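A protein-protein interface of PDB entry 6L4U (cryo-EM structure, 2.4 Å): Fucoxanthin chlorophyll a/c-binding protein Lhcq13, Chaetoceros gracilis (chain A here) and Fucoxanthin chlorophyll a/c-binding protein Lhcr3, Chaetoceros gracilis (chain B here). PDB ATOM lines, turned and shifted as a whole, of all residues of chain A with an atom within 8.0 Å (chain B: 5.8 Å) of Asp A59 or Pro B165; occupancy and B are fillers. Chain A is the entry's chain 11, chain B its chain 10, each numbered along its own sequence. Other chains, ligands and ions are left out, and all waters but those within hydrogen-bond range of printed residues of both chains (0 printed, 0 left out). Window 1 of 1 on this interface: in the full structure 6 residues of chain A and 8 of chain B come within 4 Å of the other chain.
The side-chain amide nitrogen (NE2) of Gln A61 is in hydrogen-bond range of the backbone carbonyl oxygen (O) of Gly B162, 3.1 Å away. The backbone carbonyl oxygen of Tyr B164 is in hydrogen-bond range of the side-chain amide nitrogen of Gln A61, at 2.6 Å.
O of Pro B165 is in hydrogen-bond range of NE2 of Gln B171 (2.7 Å). NZ of Lys B170 is in salt-bridge range of OD2 of Asp B167, at 2.7 Å.
O of Asp A59 touches CB of Pro B165, at 3.3 Å. Asp A59 touches Lys B170. Gly B162 touches Ala A60 (O to CB, 3.8 Å). Thr B166 touches Ala A60 (CG2 to O, 3.9 Å). CG2 of Thr B166 touches CG of Gln A61, at 3.998 Å. Gly B162 touches Ala A64 (O to CB, 3.3 Å).
Asp A59 touches two residues of chain B. Of chain A, only Asp A59 (3.3 Å) comes within 4 Å of Pro B165. Of the printed residues of chain B, Ala A64 touches Gly B162 (3.3 Å). Of the printed residues of chain B, Gln A61 touches Gly B162, Tyr B164 and Thr B166. Of the printed residues of chain A, Lys B170 touches Asp A59. Printed residues of chain A within 4 Å of Tyr B164: Gln A61. Printed residues of chain A within 4 Å of Gly B162: Ala A60, Gln A61 and Ala A64. Ala A54 touches none of the printed residues of chain B. The nearest residue of chain A that does not touch Pro B165 is Ala A60 (4.5 Å).
Printed residues of chain A that touch a printed residue of chain B: Asp A59, Ala A60, Gln A61 and Ala A64. Hydrophobic or aromatic side chains of chain A that line the printed part of chain B: Ala A60 and Ala A64. Hydrophobic or aromatic side chains of chain B within 4 Å of the printed part of chain A: Tyr B164 and Pro B165.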
ATOM      1  N   SER A  34     -18.749 -23.087  24.179  1.00  0.00           N
ATOM      2  CA  SER A  34     -18.170 -21.805  23.792  1.00  0.00           C
ATOM      3  C   SER A  34     -17.101 -21.375  24.788  1.00  0.00           C
ATOM      4  O   SER A  34     -16.148 -20.686  24.427  1.00  0.00           O
ATOM      5  CB  SER A  34     -19.257 -20.735  23.688  1.00  0.00           C
ATOM      6  OG  SER A  34     -19.830 -20.472  24.956  1.00  0.00           O
ATOM      7  N   ILE A  35     -17.269 -21.789  26.044  1.00  0.00           N
ATOM      8  CA  ILE A  35     -16.261 -21.505  27.059  1.00  0.00           C
ATOM      9  C   ILE A  35     -15.000 -22.337  26.823  1.00  0.00           C
ATOM     10  O   ILE A  35     -13.888 -21.889  27.133  1.00  0.00           O
ATOM     11  CB  ILE A  35     -16.860 -21.710  28.468  1.00  0.00           C
ATOM     12  CG1 ILE A  35     -15.890 -21.267  29.570  1.00  0.00           C
ATOM     13  CG2 ILE A  35     -17.331 -23.148  28.683  1.00  0.00           C
ATOM     14  CD1 ILE A  35     -15.566 -19.796  29.553  1.00  0.00           C
ATOM     15  N   ALA A  54     -16.077 -24.828  34.038  1.00  0.00           N
ATOM     16  CA  ALA A  54     -16.838 -24.904  32.801  1.00  0.00           C
ATOM     17  C   ALA A  54     -18.334 -24.946  33.053  1.00  0.00           C
ATOM     18  O   ALA A  54     -19.096 -24.410  32.243  1.00  0.00           O
ATOM     19  CB  ALA A  54     -16.430 -26.136  31.994  1.00  0.00           C
ATOM     20  N   ARG A  55     -18.758 -25.552  34.167  1.00  0.00           N
ATOM     21  CA  ARG A  55     -20.165 -25.799  34.459  1.00  0.00           C
ATOM     22  C   ARG A  55     -20.979 -24.525  34.635  1.00  0.00           C
ATOM     23  O   ARG A  55     -22.180 -24.535  34.344  1.00  0.00           O
ATOM     24  CB  ARG A  55     -20.298 -26.691  35.692  1.00  0.00           C
ATOM     25  CG  ARG A  55     -20.485 -28.163  35.342  1.00  0.00           C
ATOM     26  CD  ARG A  55     -20.985 -28.976  36.525  1.00  0.00           C
ATOM     27  NE  ARG A  55     -21.413 -30.315  36.127  1.00  0.00           N
ATOM     28  CZ  ARG A  55     -21.010 -31.438  36.713  1.00  0.00           C
ATOM     29  NH1 ARG A  55     -20.158 -31.393  37.728  1.00  0.00           N
ATOM     30  NH2 ARG A  55     -21.460 -32.609  36.282  1.00  0.00           N
ATOM     31  N   ILE A  56     -20.363 -23.433  35.073  1.00  0.00           N
ATOM     32  CA  ILE A  56     -21.108 -22.197  35.253  1.00  0.00           C
ATOM     33  C   ILE A  56     -21.381 -21.481  33.929  1.00  0.00           C
ATOM     34  O   ILE A  56     -22.278 -20.634  33.864  1.00  0.00           O
ATOM     35  CB  ILE A  56     -20.366 -21.277  36.237  1.00  0.00           C
ATOM     36  CG1 ILE A  56     -19.014 -20.865  35.662  1.00  0.00           C
ATOM     37  CG2 ILE A  56     -20.169 -21.983  37.566  1.00  0.00           C
ATOM     38  CD1 ILE A  56     -18.343 -19.745  36.411  1.00  0.00           C
ATOM     39  N   LEU A  57     -20.639 -21.796  32.864  1.00  0.00           N
ATOM     40  CA  LEU A  57     -20.720 -21.015  31.634  1.00  0.00           C
ATOM     41  C   LEU A  57     -20.964 -21.826  30.365  1.00  0.00           C
ATOM     42  O   LEU A  57     -20.563 -21.372  29.286  1.00  0.00           O
ATOM     43  CB  LEU A  57     -19.453 -20.177  31.448  1.00  0.00           C
ATOM     44  CG  LEU A  57     -19.227 -19.035  32.436  1.00  0.00           C
ATOM     45  CD1 LEU A  57     -17.919 -18.320  32.145  1.00  0.00           C
ATOM     46  CD2 LEU A  57     -20.397 -18.069  32.409  1.00  0.00           C
ATOM     47  N   GLU A  58     -21.586 -23.008  30.436  1.00  0.00           N
ATOM     48  CA  GLU A  58     -22.011 -23.611  29.175  1.00  0.00           C
ATOM     49  C   GLU A  58     -23.188 -22.869  28.566  1.00  0.00           C
ATOM     50  O   GLU A  58     -23.078 -22.343  27.452  1.00  0.00           O
ATOM     51  CB  GLU A  58     -22.401 -25.081  29.325  1.00  0.00           C
ATOM     52  CG  GLU A  58     -21.269 -26.028  29.610  1.00  0.00           C
ATOM     53  CD  GLU A  58     -21.171 -26.363  31.067  1.00  0.00           C
ATOM     54  OE1 GLU A  58     -22.079 -25.953  31.821  1.00  0.00           O
ATOM     55  OE2 GLU A  58     -20.194 -27.039  31.453  1.00  0.00           O
ATOM     56  N   ASP A  59     -24.306 -22.810  29.280  1.00  0.00           N
ATOM     57  CA  ASP A  59     -25.502 -22.143  28.790  1.00  0.00           C
ATOM     58  C   ASP A  59     -25.527 -20.690  29.237  1.00  0.00           C
ATOM     59  O   ASP A  59     -26.335 -20.305  30.088  1.00  0.00           O
ATOM     60  CB  ASP A  59     -26.747 -22.882  29.274  1.00  0.00           C
ATOM     61  CG  ASP A  59     -26.637 -23.330  30.721  1.00  0.00           C
ATOM     62  OD1 ASP A  59     -27.638 -23.215  31.461  1.00  0.00           O
ATOM     63  OD2 ASP A  59     -25.551 -23.798  31.120  1.00  0.00           O
ATOM     64  N   ALA A  60     -24.642 -19.877  28.672  1.00  0.00           N
ATOM     65  CA  ALA A  60     -24.557 -18.475  29.042  1.00  0.00           C
ATOM     66  C   ALA A  60     -24.219 -17.657  27.804  1.00  0.00           C
ATOM     67  O   ALA A  60     -23.817 -18.191  26.768  1.00  0.00           O
ATOM     68  CB  ALA A  60     -23.525 -18.257  30.152  1.00  0.00           C
ATOM     69  N   GLN A  61     -24.380 -16.345  27.931  1.00  0.00           N
ATOM     70  CA  GLN A  61     -24.204 -15.443  26.809  1.00  0.00           C
ATOM     71  C   GLN A  61     -22.717 -15.201  26.546  1.00  0.00           C
ATOM     72  O   GLN A  61     -21.874 -15.496  27.395  1.00  0.00           O
ATOM     73  CB  GLN A  61     -24.927 -14.130  27.100  1.00  0.00           C
ATOM     74  CG  GLN A  61     -26.434 -14.238  26.999  1.00  0.00           C
ATOM     75  CD  GLN A  61     -27.139 -13.273  27.922  1.00  0.00           C
ATOM     76  OE1 GLN A  61     -27.398 -12.126  27.560  1.00  0.00           O
ATOM     77  NE2 GLN A  61     -27.448 -13.729  29.129  1.00  0.00           N
ATOM     78  N   PRO A  62     -22.363 -14.689  25.359  1.00  0.00           N
ATOM     79  CA  PRO A  62     -20.971 -14.259  25.142  1.00  0.00           C
ATOM     80  C   PRO A  62     -20.545 -13.091  26.016  1.00  0.00           C
ATOM     81  O   PRO A  62     -19.341 -12.883  26.197  1.00  0.00           O
ATOM     82  CB  PRO A  62     -20.949 -13.880  23.657  1.00  0.00           C
ATOM     83  CG  PRO A  62     -22.017 -14.701  23.054  1.00  0.00           C
ATOM     84  CD  PRO A  62     -23.099 -14.795  24.085  1.00  0.00           C
ATOM     85  N   ALA A  64     -21.198 -13.167  29.145  1.00  0.00           N
ATOM     86  CA  ALA A  64     -20.833 -13.819  30.395  1.00  0.00           C
ATOM     87  C   ALA A  64     -19.384 -14.275  30.390  1.00  0.00           C
ATOM     88  O   ALA A  64     -18.700 -14.168  31.413  1.00  0.00           O
ATOM     89  CB  ALA A  64     -21.755 -15.004  30.663  1.00  0.00           C
ATOM     90  N   GLY B 162     -24.578 -11.750  32.533  1.00  0.00           N
ATOM     91  CA  GLY B 162     -24.923 -12.535  31.360  1.00  0.00           C
ATOM     92  C   GLY B 162     -25.286 -13.979  31.621  1.00  0.00           C
ATOM     93  O   GLY B 162     -25.089 -14.824  30.745  1.00  0.00           O
ATOM     94  N   LEU B 163     -25.833 -14.290  32.793  1.00  0.00           N
ATOM     95  CA  LEU B 163     -26.073 -15.679  33.161  1.00  0.00           C
ATOM     96  C   LEU B 163     -27.394 -16.227  32.641  1.00  0.00           C
ATOM     97  O   LEU B 163     -27.675 -17.411  32.854  1.00  0.00           O
ATOM     98  CB  LEU B 163     -26.009 -15.829  34.681  1.00  0.00           C
ATOM     99  CG  LEU B 163     -24.648 -15.488  35.288  1.00  0.00           C
ATOM    100  CD1 LEU B 163     -24.626 -15.807  36.767  1.00  0.00           C
ATOM    101  CD2 LEU B 163     -23.535 -16.227  34.565  1.00  0.00           C
ATOM    102  N   TYR B 164     -28.204 -15.416  31.983  1.00  0.00           N
ATOM    103  CA  TYR B 164     -29.414 -15.914  31.342  1.00  0.00           C
ATOM    104  C   TYR B 164     -29.028 -16.710  30.105  1.00  0.00           C
ATOM    105  O   TYR B 164     -28.314 -16.180  29.244  1.00  0.00           O
ATOM    106  CB  TYR B 164     -30.327 -14.754  30.970  1.00  0.00           C
ATOM    107  CG  TYR B 164     -31.786 -15.104  30.818  1.00  0.00           C
ATOM    108  CD1 TYR B 164     -32.426 -15.922  31.739  1.00  0.00           C
ATOM    109  CD2 TYR B 164     -32.529 -14.593  29.765  1.00  0.00           C
ATOM    110  CE1 TYR B 164     -33.764 -16.229  31.609  1.00  0.00           C
ATOM    111  CE2 TYR B 164     -33.864 -14.897  29.624  1.00  0.00           C
ATOM    112  CZ  TYR B 164     -34.477 -15.714  30.549  1.00  0.00           C
ATOM    113  OH  TYR B 164     -35.809 -16.017  30.406  1.00  0.00           O
ATOM    114  N   PRO B 165     -29.443 -17.971  29.984  1.00  0.00           N
ATOM    115  CA  PRO B 165     -29.051 -18.778  28.822  1.00  0.00           C
ATOM    116  C   PRO B 165     -29.709 -18.285  27.543  1.00  0.00           C
ATOM    117  O   PRO B 165     -30.746 -17.626  27.547  1.00  0.00           O
ATOM    118  CB  PRO B 165     -29.531 -20.186  29.186  1.00  0.00           C
ATOM    119  CG  PRO B 165     -30.568 -19.981  30.229  1.00  0.00           C
ATOM    120  CD  PRO B 165     -30.157 -18.768  30.993  1.00  0.00           C
ATOM    121  N   THR B 166     -29.066 -18.610  26.424  1.00  0.00           N
ATOM    122  CA  THR B 166     -29.537 -18.144  25.126  1.00  0.00           C
ATOM    123  C   THR B 166     -30.648 -19.021  24.562  1.00  0.00           C
ATOM    124  O   THR B 166     -31.581 -18.504  23.940  1.00  0.00           O
ATOM    125  CB  THR B 166     -28.373 -18.077  24.135  1.00  0.00           C
ATOM    126  OG1 THR B 166     -28.081 -19.392  23.647  1.00  0.00           O
ATOM    127  CG2 THR B 166     -27.137 -17.510  24.812  1.00  0.00           C
ATOM    128  N   ASP B 167     -30.564 -20.341  24.762  1.00  0.00           N
ATOM    129  CA  ASP B 167     -31.623 -21.220  24.284  1.00  0.00           C
ATOM    130  C   ASP B 167     -32.858 -21.080  25.176  1.00  0.00           C
ATOM    131  O   ASP B 167     -32.729 -20.896  26.389  1.00  0.00           O
ATOM    132  CB  ASP B 167     -31.147 -22.675  24.251  1.00  0.00           C
ATOM    133  CG  ASP B 167     -30.810 -23.213  25.619  1.00  0.00           C
ATOM    134  OD1 ASP B 167     -30.059 -22.541  26.356  1.00  0.00           O
ATOM    135  OD2 ASP B 167     -31.291 -24.316  25.952  1.00  0.00           O
ATOM    136  N   PRO B 168     -34.064 -21.139  24.602  1.00  0.00           N
ATOM    137  CA  PRO B 168     -35.260 -20.764  25.373  1.00  0.00           C
ATOM    138  C   PRO B 168     -35.798 -21.851  26.289  1.00  0.00           C
ATOM    139  O   PRO B 168     -36.486 -21.513  27.261  1.00  0.00           O
ATOM    140  CB  PRO B 168     -36.276 -20.417  24.282  1.00  0.00           C
ATOM    141  CG  PRO B 168     -35.875 -21.264  23.132  1.00  0.00           C
ATOM    142  CD  PRO B 168     -34.376 -21.353  23.177  1.00  0.00           C
ATOM    143  N   LYS B 170     -34.410 -23.858  28.458  1.00  0.00           N
ATOM    144  CA  LYS B 170     -33.891 -23.837  29.816  1.00  0.00           C
ATOM    145  C   LYS B 170     -33.855 -22.436  30.399  1.00  0.00           C
ATOM    146  O   LYS B 170     -33.455 -22.273  31.558  1.00  0.00           O
ATOM    147  CB  LYS B 170     -32.497 -24.465  29.878  1.00  0.00           C
ATOM    148  CG  LYS B 170     -31.434 -23.683  29.168  1.00  0.00           C
ATOM    149  CD  LYS B 170     -30.084 -24.296  29.451  1.00  0.00           C
ATOM    150  CE  LYS B 170     -29.950 -25.678  28.836  1.00  0.00           C
ATOM    151  NZ  LYS B 170     -29.446 -25.615  27.437  1.00  0.00           N
ATOM    152  N   GLN B 171     -34.242 -21.421  29.624  1.00  0.00           N
ATOM    153  CA  GLN B 171     -34.626 -20.147  30.215  1.00  0.00           C
ATOM    154  C   GLN B 171     -35.834 -20.306  31.119  1.00  0.00           C
ATOM    155  O   GLN B 171     -35.929 -19.637  32.153  1.00  0.00           O
ATOM    156  CB  GLN B 171     -34.945 -19.128  29.126  1.00  0.00           C
ATOM    157  CG  GLN B 171     -33.744 -18.510  28.471  1.00  0.00           C
ATOM    158  CD  GLN B 171     -34.129 -17.603  27.326  1.00  0.00           C
ATOM    159  OE1 GLN B 171     -35.253 -17.658  26.830  1.00  0.00           O
ATOM    160  NE2 GLN B 171     -33.202 -16.754  26.903  1.00  0.00           N
ATOM    161  N   MET B 174     -34.690 -21.807  34.227  1.00  0.00           N
ATOM    162  CA  MET B 174     -33.987 -20.767  34.965  1.00  0.00           C
ATOM    163  C   MET B 174     -34.977 -19.818  35.627  1.00  0.00           C
ATOM    164  O   MET B 174     -34.758 -19.370  36.759  1.00  0.00           O
ATOM    165  CB  MET B 174     -33.045 -20.007  34.032  1.00  0.00           C
ATOM    166  CG  MET B 174     -32.179 -18.982  34.726  1.00  0.00           C
ATOM    167  SD  MET B 174     -30.918 -19.713  35.778  1.00  0.00           S
ATOM    168  CE  MET B 174     -29.477 -19.527  34.734  1.00  0.00           C
